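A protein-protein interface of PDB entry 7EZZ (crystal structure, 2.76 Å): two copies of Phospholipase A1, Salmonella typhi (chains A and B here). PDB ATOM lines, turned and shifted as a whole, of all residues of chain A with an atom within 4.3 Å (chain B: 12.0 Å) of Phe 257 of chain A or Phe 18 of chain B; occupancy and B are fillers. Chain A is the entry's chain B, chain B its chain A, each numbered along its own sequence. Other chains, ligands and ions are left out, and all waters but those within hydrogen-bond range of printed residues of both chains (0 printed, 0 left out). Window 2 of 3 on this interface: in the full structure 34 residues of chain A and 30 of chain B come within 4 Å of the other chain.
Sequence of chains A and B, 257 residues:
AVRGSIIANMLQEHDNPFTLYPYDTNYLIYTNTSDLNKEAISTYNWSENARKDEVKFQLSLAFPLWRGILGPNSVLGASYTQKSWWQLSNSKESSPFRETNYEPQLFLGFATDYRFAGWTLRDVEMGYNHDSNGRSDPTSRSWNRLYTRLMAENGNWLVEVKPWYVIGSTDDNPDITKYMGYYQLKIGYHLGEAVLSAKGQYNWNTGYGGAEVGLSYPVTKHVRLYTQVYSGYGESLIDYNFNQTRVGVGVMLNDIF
A ring nitrogen (NE2) of His 190 of chain A lies within hydrogen-bond range of the chain-end carboxylate (OXT) of Phe 257 of chain A, at 3.3 Å.
1 position is printed for both chains.
Of the 5 pairs that touch across the chains among the printed residues, none has its exchanged pair printed and touching as well.
No residue of chain B comes within 4 Å of Arg 3 of chain A.
No residue of chain B comes within 4 Å of Gly 4 of chain A.
Asn 9 of chain A touches just one residue of chain B: Phe 18.
Pro 22 of chain A touches two residues of chain B.
No residue of chain B comes within 4 Å of Leu 158 of chain A.
No residue of chain B comes within 4 Å of Gly 188 of chain A.
No residue of chain B comes within 4 Å of Val 195 of chain A.
No residue of chain B comes within 4 Å of Asn 254 of chain A.
Of chain B, only Phe 18 comes within 4 Å of Asp 255 of chain A.
Of the printed residues of chain B, Phe 257 of chain A touches Phe 18 (3.8 Å).
Phe 18 of chain B touches just these residues of chain A: Asn 9, Pro 22, Asp 255 and Phe 257.
Of the printed residues of chain A, Leu 20 of chain B touches Pro 22 (3.8 Å).
The nearest residue of chain B that does not touch Phe 257 of chain A is Pro 17 of chain B (6.3 Å).
The nearest printed residue of chain A that does not touch Leu 20 of chain B is Asn 254 of chain A (4.7 Å).
Among the printed residues, merely in contact across the chains: Pro 22 of chain A with Phe 18 of chain B, Asp 255 of chain A with Phe 18 of chain B, Phe 257 of chain A with Phe 18 of chain B and Pro 22 of chain A with Leu 20 of chain B.
Of the 14 printed residues of chain B, 2 touch a printed residue of chain A.
Printed residues of chain B that touch a printed residue of chain A: Phe 18 and Leu 20.
Among the printed residues, 5 pairs touch across the chains.
The side-chain amide nitrogen of Asn 9 of chain A lies within hydrogen-bond range of the backbone carbonyl oxygen of Phe 18 of chain B (3.2 Å).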
ATOM      1  N   ARG A   3      25.097   5.200 -35.549  1.00  0.00           N
ATOM      2  CA  ARG A   3      25.266   4.393 -34.350  1.00  0.00           C
ATOM      3  C   ARG A   3      26.480   3.486 -34.552  1.00  0.00           C
ATOM      4  O   ARG A   3      26.515   2.677 -35.480  1.00  0.00           O
ATOM      5  CB  ARG A   3      23.980   3.632 -33.985  1.00  0.00           C
ATOM      6  N   GLY A   4      27.493   3.640 -33.695  1.00  0.00           N
ATOM      7  CA  GLY A   4      28.676   2.795 -33.798  1.00  0.00           C
ATOM      8  C   GLY A   4      29.904   3.500 -34.380  1.00  0.00           C
ATOM      9  O   GLY A   4      31.025   3.026 -34.183  1.00  0.00           O
ATOM     10  N   ASN A   9      31.151  10.395 -34.001  1.00  0.00           N
ATOM     11  CA  ASN A   9      30.864  10.854 -32.654  1.00  0.00           C
ATOM     12  C   ASN A   9      31.862  11.943 -32.265  1.00  0.00           C
ATOM     13  O   ASN A   9      31.479  13.010 -31.753  1.00  0.00           O
ATOM     14  CB  ASN A   9      30.878   9.675 -31.684  1.00  0.00           C
ATOM     15  CG  ASN A   9      30.284   9.975 -30.324  1.00  0.00           C
ATOM     16  OD1 ASN A   9      29.139  10.403 -30.202  1.00  0.00           O
ATOM     17  ND2 ASN A   9      31.047   9.696 -29.283  1.00  0.00           N
ATOM     18  N   PRO A  22      33.337   8.031 -25.739  1.00  0.00           N
ATOM     19  CA  PRO A  22      33.864   6.706 -25.542  1.00  0.00           C
ATOM     20  C   PRO A  22      34.520   6.217 -26.837  1.00  0.00           C
ATOM     21  O   PRO A  22      34.204   6.713 -27.853  1.00  0.00           O
ATOM     22  CB  PRO A  22      32.577   5.947 -25.279  1.00  0.00           C
ATOM     23  CG  PRO A  22      31.635   6.571 -26.224  1.00  0.00           C
ATOM     24  CD  PRO A  22      31.936   8.040 -26.101  1.00  0.00           C
ATOM     25  N   ASN A 156      21.178  -4.251 -39.748  1.00  0.00           N
ATOM     26  CA  ASN A 156      21.347  -4.490 -38.323  1.00  0.00           C
ATOM     27  C   ASN A 156      22.768  -4.938 -37.989  1.00  0.00           C
ATOM     28  O   ASN A 156      23.059  -5.197 -36.816  1.00  0.00           O
ATOM     29  CB  ASN A 156      20.381  -5.546 -37.806  1.00  0.00           C
ATOM     30  CG  ASN A 156      18.942  -5.095 -37.835  1.00  0.00           C
ATOM     31  OD1 ASN A 156      18.637  -3.930 -37.568  1.00  0.00           O
ATOM     32  ND2 ASN A 156      18.059  -6.032 -38.132  1.00  0.00           N
ATOM     33  N   LEU A 158      27.086  -4.579 -37.998  1.00  0.00           N
ATOM     34  CA  LEU A 158      28.288  -3.763 -38.010  1.00  0.00           C
ATOM     35  C   LEU A 158      29.475  -4.730 -38.068  1.00  0.00           C
ATOM     36  O   LEU A 158      29.453  -5.766 -37.399  1.00  0.00           O
ATOM     37  CB  LEU A 158      28.268  -2.925 -36.735  1.00  0.00           C
ATOM     38  CG  LEU A 158      29.476  -2.033 -36.441  1.00  0.00           C
ATOM     39  CD1 LEU A 158      29.032  -0.766 -35.685  1.00  0.00           C
ATOM     40  CD2 LEU A 158      30.530  -2.794 -35.638  1.00  0.00           C
ATOM     41  N   GLY A 188      29.033  -6.826 -34.835  1.00  0.00           N
ATOM     42  CA  GLY A 188      27.933  -6.400 -33.981  1.00  0.00           C
ATOM     43  C   GLY A 188      26.599  -6.679 -34.654  1.00  0.00           C
ATOM     44  O   GLY A 188      26.490  -6.558 -35.869  1.00  0.00           O
ATOM     45  N   TYR A 189      25.599  -7.078 -33.866  1.00  0.00           N
ATOM     46  CA  TYR A 189      24.261  -7.325 -34.385  1.00  0.00           C
ATOM     47  C   TYR A 189      23.205  -6.658 -33.497  1.00  0.00           C
ATOM     48  O   TYR A 189      23.143  -6.927 -32.298  1.00  0.00           O
ATOM     49  CB  TYR A 189      24.002  -8.821 -34.593  1.00  0.00           C
ATOM     50  CG  TYR A 189      22.707  -9.035 -35.329  1.00  0.00           C
ATOM     51  CD1 TYR A 189      22.606  -8.709 -36.664  1.00  0.00           C
ATOM     52  CD2 TYR A 189      21.559  -9.472 -34.687  1.00  0.00           C
ATOM     53  CE1 TYR A 189      21.410  -8.829 -37.358  1.00  0.00           C
ATOM     54  CE2 TYR A 189      20.353  -9.584 -35.358  1.00  0.00           C
ATOM     55  CZ  TYR A 189      20.285  -9.296 -36.707  1.00  0.00           C
ATOM     56  OH  TYR A 189      19.107  -9.408 -37.383  1.00  0.00           O
ATOM     57  N   HIS A 190      22.365  -5.792 -34.075  1.00  0.00           N
ATOM     58  CA  HIS A 190      21.326  -5.128 -33.302  1.00  0.00           C
ATOM     59  C   HIS A 190      19.994  -5.875 -33.434  1.00  0.00           C
ATOM     60  O   HIS A 190      19.320  -5.759 -34.470  1.00  0.00           O
ATOM     61  CB  HIS A 190      21.176  -3.684 -33.769  1.00  0.00           C
ATOM     62  CG  HIS A 190      21.223  -2.696 -32.652  1.00  0.00           C
ATOM     63  ND1 HIS A 190      20.290  -2.684 -31.611  1.00  0.00           N
ATOM     64  CD2 HIS A 190      22.065  -1.661 -32.422  1.00  0.00           C
ATOM     65  CE1 HIS A 190      20.569  -1.701 -30.773  1.00  0.00           C
ATOM     66  NE2 HIS A 190      21.663  -1.053 -31.248  1.00  0.00           N
ATOM     67  N   VAL A 195      22.046  -6.074 -28.129  1.00  0.00           N
ATOM     68  CA  VAL A 195      23.221  -6.058 -28.979  1.00  0.00           C
ATOM     69  C   VAL A 195      23.994  -7.354 -28.775  1.00  0.00           C
ATOM     70  O   VAL A 195      24.400  -7.639 -27.654  1.00  0.00           O
ATOM     71  CB  VAL A 195      24.095  -4.801 -28.749  1.00  0.00           C
ATOM     72  CG1 VAL A 195      25.394  -4.850 -29.534  1.00  0.00           C
ATOM     73  CG2 VAL A 195      23.361  -3.521 -29.108  1.00  0.00           C
ATOM     74  N   ASN A 254      28.232   1.678 -22.739  1.00  0.00           N
ATOM     75  CA  ASN A 254      28.049   1.712 -24.173  1.00  0.00           C
ATOM     76  C   ASN A 254      28.472   0.364 -24.743  1.00  0.00           C
ATOM     77  O   ASN A 254      29.505  -0.172 -24.321  1.00  0.00           O
ATOM     78  CB  ASN A 254      28.882   2.844 -24.785  1.00  0.00           C
ATOM     79  CG  ASN A 254      30.375   2.686 -24.570  1.00  0.00           C
ATOM     80  OD1 ASN A 254      30.839   2.684 -23.435  1.00  0.00           O
ATOM     81  ND2 ASN A 254      31.133   2.555 -25.651  1.00  0.00           N
ATOM     82  N   ASP A 255      27.679  -0.149 -25.705  1.00  0.00           N
ATOM     83  CA  ASP A 255      28.055  -1.325 -26.474  1.00  0.00           C
ATOM     84  C   ASP A 255      28.694  -0.843 -27.778  1.00  0.00           C
ATOM     85  O   ASP A 255      28.834   0.362 -27.946  1.00  0.00           O
ATOM     86  CB  ASP A 255      26.901  -2.335 -26.558  1.00  0.00           C
ATOM     87  CG  ASP A 255      27.377  -3.774 -26.731  1.00  0.00           C
ATOM     88  OD1 ASP A 255      28.511  -3.954 -27.230  1.00  0.00           O
ATOM     89  OD2 ASP A 255      26.634  -4.722 -26.326  1.00  0.00           O
ATOM     90  N   ILE A 256      29.083  -1.760 -28.679  1.00  0.00           N
ATOM     91  CA  ILE A 256      29.727  -1.344 -29.913  1.00  0.00           C
ATOM     92  C   ILE A 256      28.799  -0.528 -30.824  1.00  0.00           C
ATOM     93  O   ILE A 256      29.297   0.329 -31.537  1.00  0.00           O
ATOM     94  CB  ILE A 256      30.491  -2.473 -30.619  1.00  0.00           C
ATOM     95  CG1 ILE A 256      29.668  -3.746 -30.817  1.00  0.00           C
ATOM     96  CG2 ILE A 256      31.766  -2.768 -29.863  1.00  0.00           C
ATOM     97  CD1 ILE A 256      30.369  -4.778 -31.698  1.00  0.00           C
ATOM     98  N   PHE A 257      27.472  -0.712 -30.772  1.00  0.00           N
ATOM     99  CA  PHE A 257      26.577   0.301 -31.334  1.00  0.00           C
ATOM    100  C   PHE A 257      25.188   0.216 -30.699  1.00  0.00           C
ATOM    101  O   PHE A 257      25.006  -0.508 -29.710  1.00  0.00           O
ATOM    102  CB  PHE A 257      26.474   0.261 -32.859  1.00  0.00           C
ATOM    103  CG  PHE A 257      25.894  -0.996 -33.445  1.00  0.00           C
ATOM    104  CD1 PHE A 257      26.016  -2.209 -32.782  1.00  0.00           C
ATOM    105  CD2 PHE A 257      25.257  -0.960 -34.674  1.00  0.00           C
ATOM    106  CE1 PHE A 257      25.500  -3.362 -33.338  1.00  0.00           C
ATOM    107  CE2 PHE A 257      24.751  -2.122 -35.236  1.00  0.00           C
ATOM    108  CZ  PHE A 257      24.874  -3.316 -34.563  1.00  0.00           C
ATOM    109  OXT PHE A 257      24.263   0.908 -31.174  1.00  0.00           O
ATOM    110  N   GLN B  12      21.525  15.938 -16.974  1.00  0.00           N
ATOM    111  CA  GLN B  12      21.335  16.399 -18.339  1.00  0.00           C
ATOM    112  C   GLN B  12      21.243  15.180 -19.257  1.00  0.00           C
ATOM    113  O   GLN B  12      21.981  14.214 -19.072  1.00  0.00           O
ATOM    114  CB  GLN B  12      22.450  17.389 -18.713  1.00  0.00           C
ATOM    115  N   GLU B  13      20.291  15.242 -20.209  1.00  0.00           N
ATOM    116  CA  GLU B  13      20.008  14.242 -21.238  1.00  0.00           C
ATOM    117  C   GLU B  13      21.222  14.013 -22.159  1.00  0.00           C
ATOM    118  O   GLU B  13      21.077  13.263 -23.159  1.00  0.00           O
ATOM    119  CB  GLU B  13      18.821  14.713 -22.087  1.00  0.00           C
ATOM    120  N   ASN B  16      25.003  10.548 -28.528  1.00  0.00           N
ATOM    121  CA  ASN B  16      23.802  10.606 -27.646  1.00  0.00           C
ATOM    122  C   ASN B  16      23.954   9.590 -26.518  1.00  0.00           C
ATOM    123  O   ASN B  16      24.071  10.021 -25.371  1.00  0.00           O
ATOM    124  CB  ASN B  16      22.501  10.318 -28.385  1.00  0.00           C
ATOM    125  CG  ASN B  16      21.288  10.604 -27.534  1.00  0.00           C
ATOM    126  OD1 ASN B  16      20.678   9.697 -26.985  1.00  0.00           O
ATOM    127  ND2 ASN B  16      20.930  11.869 -27.426  1.00  0.00           N
ATOM    128  N   PRO B  17      23.927   8.264 -26.792  1.00  0.00           N
ATOM    129  CA  PRO B  17      24.181   7.245 -25.784  1.00  0.00           C
ATOM    130  C   PRO B  17      25.685   6.934 -25.714  1.00  0.00           C
ATOM    131  O   PRO B  17      26.087   6.148 -24.919  1.00  0.00           O
ATOM    132  CB  PRO B  17      23.373   6.044 -26.284  1.00  0.00           C
ATOM    133  CG  PRO B  17      23.361   6.188 -27.770  1.00  0.00           C
ATOM    134  CD  PRO B  17      23.564   7.655 -28.065  1.00  0.00           C
ATOM    135  N   PHE B  18      26.457   7.555 -26.594  1.00  0.00           N
ATOM    136  CA  PHE B  18      27.928   7.450 -26.655  1.00  0.00           C
ATOM    137  C   PHE B  18      28.492   8.744 -26.062  1.00  0.00           C
ATOM    138  O   PHE B  18      29.322   9.416 -26.662  1.00  0.00           O
ATOM    139  CB  PHE B  18      28.343   7.136 -28.092  1.00  0.00           C
ATOM    140  CG  PHE B  18      27.617   5.954 -28.674  1.00  0.00           C
ATOM    141  CD1 PHE B  18      27.975   4.660 -28.331  1.00  0.00           C
ATOM    142  CD2 PHE B  18      26.564   6.131 -29.548  1.00  0.00           C
ATOM    143  CE1 PHE B  18      27.306   3.565 -28.849  1.00  0.00           C
ATOM    144  CE2 PHE B  18      25.896   5.031 -30.063  1.00  0.00           C
ATOM    145  CZ  PHE B  18      26.266   3.757 -29.712  1.00  0.00           C
ATOM    146  N   THR B  19      27.999   9.080 -24.882  1.00  0.00           N
ATOM    147  CA  THR B  19      28.454  10.290 -24.171  1.00  0.00           C
ATOM    148  C   THR B  19      28.747   9.908 -22.725  1.00  0.00           C
ATOM    149  O   THR B  19      27.828   9.456 -22.068  1.00  0.00           O
ATOM    150  CB  THR B  19      27.380  11.383 -24.207  1.00  0.00           C
ATOM    151  OG1 THR B  19      26.176  10.921 -23.602  1.00  0.00           O
ATOM    152  CG2 THR B  19      27.069  11.848 -25.609  1.00  0.00           C
ATOM    153  N   LEU B  20      29.986  10.057 -22.268  1.00  0.00           N
ATOM    154  CA  LEU B  20      30.308   9.760 -20.882  1.00  0.00           C
ATOM    155  C   LEU B  20      30.338  11.056 -20.066  1.00  0.00           C
ATOM    156  O   LEU B  20      30.507  12.151 -20.619  1.00  0.00           O
ATOM    157  CB  LEU B  20      31.653   9.033 -20.847  1.00  0.00           C
ATOM    158  CG  LEU B  20      31.677   7.761 -21.685  1.00  0.00           C
ATOM    159  CD1 LEU B  20      33.046   7.103 -21.693  1.00  0.00           C
ATOM    160  CD2 LEU B  20      30.630   6.804 -21.172  1.00  0.00           C
ATOM    161  N   TYR B  21      30.167  10.899 -18.760  1.00  0.00           N
ATOM    162  CA  TYR B  21      30.176  12.060 -17.848  1.00  0.00           C
ATOM    163  C   TYR B  21      31.430  12.007 -16.996  1.00  0.00           C
ATOM    164  O   TYR B  21      31.842  10.950 -16.609  1.00  0.00           O
ATOM    165  CB  TYR B  21      28.969  12.053 -16.913  1.00  0.00           C
ATOM    166  CG  TYR B  21      27.630  12.056 -17.588  1.00  0.00           C
ATOM    167  CD1 TYR B  21      27.114  10.898 -18.122  1.00  0.00           C
ATOM    168  CD2 TYR B  21      26.878  13.204 -17.682  1.00  0.00           C
ATOM    169  CE1 TYR B  21      25.882  10.865 -18.736  1.00  0.00           C
ATOM    170  CE2 TYR B  21      25.639  13.192 -18.286  1.00  0.00           C
ATOM    171  CZ  TYR B  21      25.139  12.019 -18.810  1.00  0.00           C
ATOM    172  OH  TYR B  21      23.935  11.993 -19.434  1.00  0.00           O
ATOM    173  N   PRO B  22      32.078  13.146 -16.740  1.00  0.00           N
ATOM    174  CA  PRO B  22      33.196  13.169 -15.852  1.00  0.00           C
ATOM    175  C   PRO B  22      32.717  13.463 -14.429  1.00  0.00           C
ATOM    176  O   PRO B  22      31.664  13.984 -14.239  1.00  0.00           O
ATOM    177  CB  PRO B  22      33.948  14.355 -16.438  1.00  0.00           C
ATOM    178  CG  PRO B  22      32.872  15.294 -16.752  1.00  0.00           C
ATOM    179  CD  PRO B  22      31.815  14.421 -17.367  1.00  0.00           C
ATOM    180  N   LEU B  61      35.135   9.359 -13.864  1.00  0.00           N
ATOM    181  CA  LEU B  61      33.860   9.248 -14.571  1.00  0.00           C
ATOM    182  C   LEU B  61      32.703   9.170 -13.579  1.00  0.00           C
ATOM    183  O   LEU B  61      32.821   8.537 -12.534  1.00  0.00           O
ATOM    184  CB  LEU B  61      33.834   7.957 -15.382  1.00  0.00           C
ATOM    185  CG  LEU B  61      34.764   7.829 -16.588  1.00  0.00           C
ATOM    186  CD1 LEU B  61      34.435   6.535 -17.325  1.00  0.00           C
ATOM    187  CD2 LEU B  61      34.601   9.002 -17.550  1.00  0.00           C
ATOM    188  N   ALA B  62      31.568   9.774 -13.948  1.00  0.00           N
ATOM    189  CA  ALA B  62      30.320   9.646 -13.212  1.00  0.00           C
ATOM    190  C   ALA B  62      29.362   8.770 -14.021  1.00  0.00           C
ATOM    191  O   ALA B  62      29.371   8.824 -15.240  1.00  0.00           O
ATOM    192  CB  ALA B  62      29.738  11.008 -12.921  1.00  0.00           C
ATOM    193  N   PHE B  63      28.553   7.962 -13.333  1.00  0.00           N
ATOM    194  CA  PHE B  63      27.603   7.094 -13.998  1.00  0.00           C
ATOM    195  C   PHE B  63      26.222   7.293 -13.389  1.00  0.00           C
ATOM    196  O   PHE B  63      25.937   6.775 -12.304  1.00  0.00           O
ATOM    197  CB  PHE B  63      27.971   5.613 -13.857  1.00  0.00           C
ATOM    198  CG  PHE B  63      29.431   5.305 -14.034  1.00  0.00           C
ATOM    199  CD1 PHE B  63      30.038   5.417 -15.268  1.00  0.00           C
ATOM    200  CD2 PHE B  63      30.196   4.912 -12.950  1.00  0.00           C
ATOM    201  CE1 PHE B  63      31.394   5.161 -15.411  1.00  0.00           C
ATOM    202  CE2 PHE B  63      31.546   4.654 -13.093  1.00  0.00           C
ATOM    203  CZ  PHE B  63      32.147   4.770 -14.323  1.00  0.00           C
ATOM    204  N   PRO B  64      25.314   7.990 -14.109  1.00  0.00           N
ATOM    205  CA  PRO B  64      23.919   8.099 -13.670  1.00  0.00           C
ATOM    206  C   PRO B  64      23.252   6.727 -13.791  1.00  0.00           C
ATOM    207  O   PRO B  64      23.206   6.143 -14.871  1.00  0.00           O
ATOM    208  CB  PRO B  64      23.296   9.114 -14.642  1.00  0.00           C
ATOM    209  CG  PRO B  64      24.493   9.740 -15.358  1.00  0.00           C
ATOM    210  CD  PRO B  64      25.579   8.687 -15.384  1.00  0.00           C
ATOM    211  N   ARG B  67      17.952   8.375 -12.472  1.00  0.00           N
ATOM    212  CA  ARG B  67      17.613   9.800 -12.334  1.00  0.00           C
ATOM    213  C   ARG B  67      16.187   9.915 -11.818  1.00  0.00           C
ATOM    214  O   ARG B  67      15.336   9.204 -12.291  1.00  0.00           O
ATOM    215  CB  ARG B  67      17.628  10.442 -13.713  1.00  0.00           C
ATOM    216  CG  ARG B  67      18.974  10.409 -14.406  1.00  0.00           C
ATOM    217  CD  ARG B  67      18.937  11.534 -15.398  1.00  0.00           C
ATOM    218  NE  ARG B  67      19.115  11.127 -16.766  1.00  0.00           N
ATOM    219  CZ  ARG B  67      20.219  11.331 -17.464  1.00  0.00           C
